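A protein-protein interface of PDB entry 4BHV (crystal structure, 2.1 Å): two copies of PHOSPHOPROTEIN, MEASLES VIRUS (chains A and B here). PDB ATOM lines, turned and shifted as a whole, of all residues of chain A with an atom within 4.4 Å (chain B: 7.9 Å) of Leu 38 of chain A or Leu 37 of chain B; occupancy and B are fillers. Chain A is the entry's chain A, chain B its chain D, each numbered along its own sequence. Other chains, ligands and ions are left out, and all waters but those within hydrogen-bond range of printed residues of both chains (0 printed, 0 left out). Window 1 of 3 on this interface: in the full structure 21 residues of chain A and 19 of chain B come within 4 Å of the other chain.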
ATOM      1  N   LEU A  34     -27.511   4.446 -17.983  1.00  0.00           N
ATOM      2  CA  LEU A  34     -26.175   4.841 -17.784  1.00  0.00           C
ATOM      3  C   LEU A  34     -25.163   3.883 -18.398  1.00  0.00           C
ATOM      4  O   LEU A  34     -24.212   4.366 -18.984  1.00  0.00           O
ATOM      5  CB  LEU A  34     -25.856   4.940 -16.288  1.00  0.00           C
ATOM      6  CG  LEU A  34     -26.516   6.079 -15.507  1.00  0.00           C
ATOM      7  CD1 LEU A  34     -26.145   6.042 -14.036  1.00  0.00           C
ATOM      8  CD2 LEU A  34     -26.139   7.411 -16.110  1.00  0.00           C
ATOM      9  N   GLU A  35     -25.414   2.580 -18.373  1.00  0.00           N
ATOM     10  CA  GLU A  35     -24.561   1.621 -19.062  1.00  0.00           C
ATOM     11  C   GLU A  35     -24.560   1.876 -20.564  1.00  0.00           C
ATOM     12  O   GLU A  35     -23.517   1.855 -21.190  1.00  0.00           O
ATOM     13  CB  GLU A  35     -25.021   0.195 -18.769  1.00  0.00           C
ATOM     14  CG  GLU A  35     -24.719  -0.275 -17.360  1.00  0.00           C
ATOM     15  CD  GLU A  35     -23.232  -0.367 -17.068  1.00  0.00           C
ATOM     16  OE1 GLU A  35     -22.428  -0.332 -18.011  1.00  0.00           O
ATOM     17  OE2 GLU A  35     -22.873  -0.468 -15.885  1.00  0.00           O
ATOM     18  N   SER A  36     -25.724   2.157 -21.138  1.00  0.00           N
ATOM     19  CA  SER A  36     -25.791   2.474 -22.554  1.00  0.00           C
ATOM     20  C   SER A  36     -25.006   3.744 -22.878  1.00  0.00           C
ATOM     21  O   SER A  36     -24.278   3.797 -23.861  1.00  0.00           O
ATOM     22  CB  SER A  36     -27.241   2.620 -23.007  1.00  0.00           C
ATOM     23  OG  SER A  36     -27.313   2.875 -24.391  1.00  0.00           O
ATOM     24  N   LEU A  37     -25.132   4.744 -22.013  1.00  0.00           N
ATOM     25  CA  LEU A  37     -24.479   6.035 -22.191  1.00  0.00           C
ATOM     26  C   LEU A  37     -22.957   5.905 -22.217  1.00  0.00           C
ATOM     27  O   LEU A  37     -22.286   6.596 -22.968  1.00  0.00           O
ATOM     28  CB  LEU A  37     -24.900   7.016 -21.092  1.00  0.00           C
ATOM     29  CG  LEU A  37     -26.138   7.879 -21.368  1.00  0.00           C
ATOM     30  CD1 LEU A  37     -26.480   8.767 -20.183  1.00  0.00           C
ATOM     31  CD2 LEU A  37     -25.972   8.698 -22.637  1.00  0.00           C
ATOM     32  N   LEU A  38     -22.440   4.987 -21.408  1.00  0.00           N
ATOM     33  CA  LEU A  38     -21.005   4.779 -21.241  1.00  0.00           C
ATOM     34  C   LEU A  38     -20.356   4.333 -22.546  1.00  0.00           C
ATOM     35  O   LEU A  38     -19.173   4.535 -22.748  1.00  0.00           O
ATOM     36  CB  LEU A  38     -20.719   3.783 -20.119  1.00  0.00           C
ATOM     37  CG  LEU A  38     -20.762   4.370 -18.714  1.00  0.00           C
ATOM     38  CD1 LEU A  38     -20.654   3.280 -17.661  1.00  0.00           C
ATOM     39  CD2 LEU A  38     -19.672   5.410 -18.533  1.00  0.00           C
ATOM     40  N   LEU A  39     -21.164   3.778 -23.440  1.00  0.00           N
ATOM     41  CA  LEU A  39     -20.725   3.352 -24.759  1.00  0.00           C
ATOM     42  C   LEU A  39     -20.279   4.543 -25.601  1.00  0.00           C
ATOM     43  O   LEU A  39     -19.609   4.386 -26.606  1.00  0.00           O
ATOM     44  CB  LEU A  39     -21.814   2.548 -25.477  1.00  0.00           C
ATOM     45  CG  LEU A  39     -22.256   1.253 -24.785  1.00  0.00           C
ATOM     46  CD1 LEU A  39     -23.170   0.421 -25.668  1.00  0.00           C
ATOM     47  CD2 LEU A  39     -21.076   0.429 -24.297  1.00  0.00           C
ATOM     48  N   LEU A  40     -20.641   5.737 -25.151  1.00  0.00           N
ATOM     49  CA  LEU A  40     -20.262   6.968 -25.826  1.00  0.00           C
ATOM     50  C   LEU A  40     -18.751   7.161 -25.849  1.00  0.00           C
ATOM     51  O   LEU A  40     -18.201   7.643 -26.824  1.00  0.00           O
ATOM     52  CB  LEU A  40     -20.946   8.168 -25.188  1.00  0.00           C
ATOM     53  CG  LEU A  40     -22.272   8.526 -25.853  1.00  0.00           C
ATOM     54  CD1 LEU A  40     -23.153   9.331 -24.916  1.00  0.00           C
ATOM     55  CD2 LEU A  40     -22.014   9.254 -27.160  1.00  0.00           C
ATOM     56  N   LYS A  41     -18.096   6.742 -24.778  1.00  0.00           N
ATOM     57  CA  LYS A  41     -16.672   6.957 -24.603  1.00  0.00           C
ATOM     58  C   LYS A  41     -15.859   6.287 -25.713  1.00  0.00           C
ATOM     59  O   LYS A  41     -14.929   6.877 -26.238  1.00  0.00           O
ATOM     60  CB  LYS A  41     -16.243   6.466 -23.219  1.00  0.00           C
ATOM     61  CG  LYS A  41     -16.999   7.136 -22.084  1.00  0.00           C
ATOM     62  CD  LYS A  41     -17.012   6.301 -20.819  1.00  0.00           C
ATOM     63  CE  LYS A  41     -15.667   6.357 -20.121  1.00  0.00           C
ATOM     64  NZ  LYS A  41     -15.221   7.754 -19.864  1.00  0.00           N
ATOM     65  N   LYS B  29     -23.474   3.473  -7.008  1.00  0.00           N
ATOM     66  CA  LYS B  29     -23.105   3.016  -8.340  1.00  0.00           C
ATOM     67  C   LYS B  29     -23.502   4.016  -9.414  1.00  0.00           C
ATOM     68  O   LYS B  29     -22.734   4.281 -10.323  1.00  0.00           O
ATOM     69  CB  LYS B  29     -23.717   1.648  -8.641  1.00  0.00           C
ATOM     70  CG  LYS B  29     -22.816   0.488  -8.266  1.00  0.00           C
ATOM     71  CD  LYS B  29     -23.520  -0.468  -7.335  1.00  0.00           C
ATOM     72  CE  LYS B  29     -24.436  -1.415  -8.085  1.00  0.00           C
ATOM     73  NZ  LYS B  29     -25.186  -2.269  -7.124  1.00  0.00           N
ATOM     74  N   ILE B  30     -24.691   4.587  -9.290  1.00  0.00           N
ATOM     75  CA  ILE B  30     -25.158   5.566 -10.259  1.00  0.00           C
ATOM     76  C   ILE B  30     -24.218   6.773 -10.269  1.00  0.00           C
ATOM     77  O   ILE B  30     -23.886   7.297 -11.320  1.00  0.00           O
ATOM     78  CB  ILE B  30     -26.596   6.027  -9.948  1.00  0.00           C
ATOM     79  CG1 ILE B  30     -27.603   4.937 -10.306  1.00  0.00           C
ATOM     80  CG2 ILE B  30     -26.937   7.313 -10.691  1.00  0.00           C
ATOM     81  CD1 ILE B  30     -28.895   5.035  -9.537  1.00  0.00           C
ATOM     82  N   ILE B  31     -23.789   7.191  -9.087  1.00  0.00           N
ATOM     83  CA  ILE B  31     -22.846   8.289  -8.957  1.00  0.00           C
ATOM     84  C   ILE B  31     -21.487   7.973  -9.594  1.00  0.00           C
ATOM     85  O   ILE B  31     -20.925   8.802 -10.299  1.00  0.00           O
ATOM     86  CB  ILE B  31     -22.668   8.715  -7.485  1.00  0.00           C
ATOM     87  CG1 ILE B  31     -23.891   9.492  -7.004  1.00  0.00           C
ATOM     88  CG2 ILE B  31     -21.417   9.563  -7.319  1.00  0.00           C
ATOM     89  CD1 ILE B  31     -23.991   9.635  -5.506  1.00  0.00           C
ATOM     90  N   SER B  32     -20.992   6.753  -9.386  1.00  0.00           N
ATOM     91  CA  SER B  32     -19.713   6.347  -9.957  1.00  0.00           C
ATOM     92  C   SER B  32     -19.775   6.381 -11.479  1.00  0.00           C
ATOM     93  O   SER B  32     -18.854   6.850 -12.131  1.00  0.00           O
ATOM     94  CB  SER B  32     -19.317   4.944  -9.489  1.00  0.00           C
ATOM     95  OG  SER B  32     -19.216   4.867  -8.087  1.00  0.00           O
ATOM     96  N   LYS B  33     -20.872   5.886 -12.036  1.00  0.00           N
ATOM     97  CA  LYS B  33     -21.072   5.997 -13.497  1.00  0.00           C
ATOM     98  C   LYS B  33     -21.159   7.492 -14.064  1.00  0.00           C
ATOM     99  O   LYS B  33     -20.542   7.762 -15.078  1.00  0.00           O
ATOM    100  CB  LYS B  33     -22.329   5.210 -13.880  1.00  0.00           C
ATOM    101  CG  LYS B  33     -22.179   3.700 -13.758  1.00  0.00           C
ATOM    102  CD  LYS B  33     -23.528   2.997 -13.859  1.00  0.00           C
ATOM    103  CE  LYS B  33     -23.379   1.477 -13.858  1.00  0.00           C
ATOM    104  NZ  LYS B  33     -22.742   0.957 -12.617  1.00  0.00           N
ATOM    105  N   LEU B  34     -21.833   8.387 -13.354  1.00  0.00           N
ATOM    106  CA  LEU B  34     -21.934   9.788 -13.741  1.00  0.00           C
ATOM    107  C   LEU B  34     -20.574  10.480 -13.751  1.00  0.00           C
ATOM    108  O   LEU B  34     -20.291  11.284 -14.619  1.00  0.00           O
ATOM    109  CB  LEU B  34     -22.904  10.530 -12.828  1.00  0.00           C
ATOM    110  CG  LEU B  34     -24.383  10.248 -13.068  1.00  0.00           C
ATOM    111  CD1 LEU B  34     -25.245  10.786 -11.942  1.00  0.00           C
ATOM    112  CD2 LEU B  34     -24.820  10.797 -14.410  1.00  0.00           C
ATOM    113  N   GLU B  35     -19.738  10.154 -12.771  1.00  0.00           N
ATOM    114  CA  GLU B  35     -18.399  10.709 -12.709  1.00  0.00           C
ATOM    115  C   GLU B  35     -17.576  10.277 -13.928  1.00  0.00           C
ATOM    116  O   GLU B  35     -16.855  11.074 -14.505  1.00  0.00           O
ATOM    117  CB  GLU B  35     -17.724  10.313 -11.402  1.00  0.00           C
ATOM    118  CG  GLU B  35     -18.391  10.900 -10.171  1.00  0.00           C
ATOM    119  CD  GLU B  35     -18.229  12.406 -10.074  1.00  0.00           C
ATOM    120  OE1 GLU B  35     -17.664  13.013 -10.998  1.00  0.00           O
ATOM    121  OE2 GLU B  35     -18.662  12.979  -9.064  1.00  0.00           O
ATOM    122  N   SER B  36     -17.713   9.016 -14.327  1.00  0.00           N
ATOM    123  CA  SER B  36     -17.040   8.515 -15.519  1.00  0.00           C
ATOM    124  C   SER B  36     -17.514   9.212 -16.796  1.00  0.00           C
ATOM    125  O   SER B  36     -16.718   9.560 -17.650  1.00  0.00           O
ATOM    126  CB  SER B  36     -17.222   7.005 -15.646  1.00  0.00           C
ATOM    127  OG  SER B  36     -16.653   6.525 -16.842  1.00  0.00           O
ATOM    128  N   LEU B  37     -18.816   9.436 -16.899  1.00  0.00           N
ATOM    129  CA  LEU B  37     -19.398  10.128 -18.046  1.00  0.00           C
ATOM    130  C   LEU B  37     -18.885  11.563 -18.168  1.00  0.00           C
ATOM    131  O   LEU B  37     -18.700  12.066 -19.265  1.00  0.00           O
ATOM    132  CB  LEU B  37     -20.927  10.083 -18.004  1.00  0.00           C
ATOM    133  CG  LEU B  37     -21.553   8.776 -18.489  1.00  0.00           C
ATOM    134  CD1 LEU B  37     -23.008   8.684 -18.060  1.00  0.00           C
ATOM    135  CD2 LEU B  37     -21.425   8.623 -19.997  1.00  0.00           C
ATOM    136  N   LEU B  38     -18.618  12.186 -17.029  1.00  0.00           N
ATOM    137  CA  LEU B  38     -18.209  13.583 -16.961  1.00  0.00           C
ATOM    138  C   LEU B  38     -16.894  13.839 -17.691  1.00  0.00           C
ATOM    139  O   LEU B  38     -16.693  14.900 -18.272  1.00  0.00           O
ATOM    140  CB  LEU B  38     -18.148  14.073 -15.511  1.00  0.00           C
ATOM    141  CG  LEU B  38     -19.491  14.557 -14.962  1.00  0.00           C
ATOM    142  CD1 LEU B  38     -19.503  14.516 -13.449  1.00  0.00           C
ATOM    143  CD2 LEU B  38     -19.824  15.945 -15.476  1.00  0.00           C
ATOM    144  N   LEU B  39     -16.038  12.828 -17.710  1.00  0.00           N
ATOM    145  CA  LEU B  39     -14.731  12.916 -18.343  1.00  0.00           C
ATOM    146  C   LEU B  39     -14.901  13.123 -19.846  1.00  0.00           C
ATOM    147  O   LEU B  39     -13.972  13.500 -20.537  1.00  0.00           O
ATOM    148  CB  LEU B  39     -13.878  11.681 -18.039  1.00  0.00           C
ATOM    149  CG  LEU B  39     -13.691  11.305 -16.569  1.00  0.00           C
ATOM    150  CD1 LEU B  39     -12.964   9.980 -16.456  1.00  0.00           C
ATOM    151  CD2 LEU B  39     -12.959  12.386 -15.785  1.00  0.00           C
ATOM    152  N   LEU B  40     -16.123  12.919 -20.317  1.00  0.00           N
ATOM    153  CA  LEU B  40     -16.481  13.163 -21.703  1.00  0.00           C
ATOM    154  C   LEU B  40     -16.287  14.631 -22.053  1.00  0.00           C
ATOM    155  O   LEU B  40     -15.952  14.952 -23.177  1.00  0.00           O
ATOM    156  CB  LEU B  40     -17.919  12.745 -21.984  1.00  0.00           C
ATOM    157  CG  LEU B  40     -18.101  11.323 -22.500  1.00  0.00           C
ATOM    158  CD1 LEU B  40     -19.569  10.992 -22.656  1.00  0.00           C
ATOM    159  CD2 LEU B  40     -17.332  11.087 -23.794  1.00  0.00           C
ATOM    160  N   LYS B  41     -16.460  15.512 -21.074  1.00  0.00           N
ATOM    161  CA  LYS B  41     -16.377  16.941 -21.331  1.00  0.00           C
ATOM    162  C   LYS B  41     -14.995  17.290 -21.867  1.00  0.00           C
ATOM    163  O   LYS B  41     -14.871  18.044 -22.820  1.00  0.00           O
ATOM    164  CB  LYS B  41     -16.654  17.734 -20.051  1.00  0.00           C
ATOM    165  CG  LYS B  41     -18.093  17.700 -19.575  1.00  0.00           C
ATOM    166  CD  LYS B  41     -18.354  18.758 -18.514  1.00  0.00           C
ATOM    167  CE  LYS B  41     -19.837  19.038 -18.374  1.00  0.00           C
ATOM    168  NZ  LYS B  41     -20.214  20.331 -18.992  1.00  0.00           N
ATOM    169  N   GLY B  42     -13.965  16.714 -21.256  1.00  0.00           N
ATOM    170  CA  GLY B  42     -12.605  16.841 -21.740  1.00  0.00           C
ATOM    171  C   GLY B  42     -12.356  16.235 -23.112  1.00  0.00           C
ATOM    172  O   GLY B  42     -11.631  16.801 -23.909  1.00  0.00           O
ATOM    173  N   GLU B  43     -12.937  15.069 -23.374  1.00  0.00           N
ATOM    174  CA  GLU B  43     -12.782  14.402 -24.666  1.00  0.00           C
ATOM    175  C   GLU B  43     -13.374  15.187 -25.833  1.00  0.00           C
ATOM    176  O   GLU B  43     -12.752  15.300 -26.878  1.00  0.00           O
ATOM    177  CB  GLU B  43     -13.405  13.008 -24.626  1.00  0.00           C
ATOM    178  CG  GLU B  43     -12.688  12.038 -23.707  1.00  0.00           C
ATOM    179  CD  GLU B  43     -11.192  12.067 -23.906  1.00  0.00           C
ATOM    180  OE1 GLU B  43     -10.721  11.659 -24.981  1.00  0.00           O
ATOM    181  OE2 GLU B  43     -10.486  12.517 -22.992  1.00  0.00           O
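The side-chain carboxylate (OE2) of Glu 35 of chain A lies within salt-bridge range of the side-chain amino group (NZ) of Lys 33 of chain B, 3.6 Å away.
The side-chain amino group (NZ) of Lys 41 of chain A lies within hydrogen-bond range of the backbone carbonyl oxygen (O) of Ser 36 of chain B, at 3.2 Å.
Among the printed residues, pairs that only touch across the chains: Leu 38 of chain A with Ser 36 of chain B (3.6 Å), Leu 34 of chain A with Ile 30 of chain B (3.7 Å), Leu 37 of chain A with Leu 37 of chain B (3.7 Å), Leu 38 of chain A with Leu 37 of chain B (3.9 Å), Leu 34 of chain A with Lys 33 of chain B (3.9 Å) and Leu 34 of chain A with Leu 37 of chain B (3.9 Å).
Of the printed residues of chain B, Leu 34 of chain A touches Ile 30, Lys 33 and Leu 37.
Printed residues of chain A within 4 Å of Lys 33 of chain B: Leu 34 (3.9 Å) and Glu 35 (2.9 Å).
Of the printed residues of chain A, Ser 36 of chain B touches Leu 38 and Lys 41.
Leu 34 of chain B touches none of the printed residues of chain A.
Gly 42 of chain B touches none of the printed residues of chain A.
The nearest printed residue of chain A that does not touch Leu 37 of chain B is Lys 41 of chain A (5.0 Å).
The nearest printed residue of chain B that does not touch Leu 34 of chain A is Leu 34 of chain B (4.01 Å).
Printed residues of chain B that touch a printed residue of chain A: Ile 30, Lys 33, Ser 36 and Leu 37.
Hydrophobic or aromatic side chains of chain B within 4 Å of the printed part of chain A: Ile 30 and Leu 37.
Hydrophobic or aromatic side chains of chain A that line the printed part of chain B: Leu 34, Leu 37 and Leu 38.
Along chain A the printed residues that touch a printed residue of chain B span positions 34 to 41.
Among the printed residues, 8 pairs touch across the chains.
Leu 37 of chain A touches its own counterpart, Leu 37 of chain B.
Leu 38 of chain A touches Ser 36 of chain B, but with the chains exchanged Ser 36 of chain A does not touch Leu 38 of chain B (12.1 Å).
Leu 38 of chain A touches Leu 37 of chain B, but with the chains exchanged Leu 37 of chain A does not touch Leu 38 of chain B (8.9 Å).
Lys 41 of chain A touches Ser 36 of chain B, but with the chains exchanged Ser 36 of chain A does not touch Lys 41 of chain B (14.4 Å).
8 positions are printed for both chains.
Of the 8 pairs that touch across the chains among the printed residues, 1 has its exchanged pair printed and touching as well.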
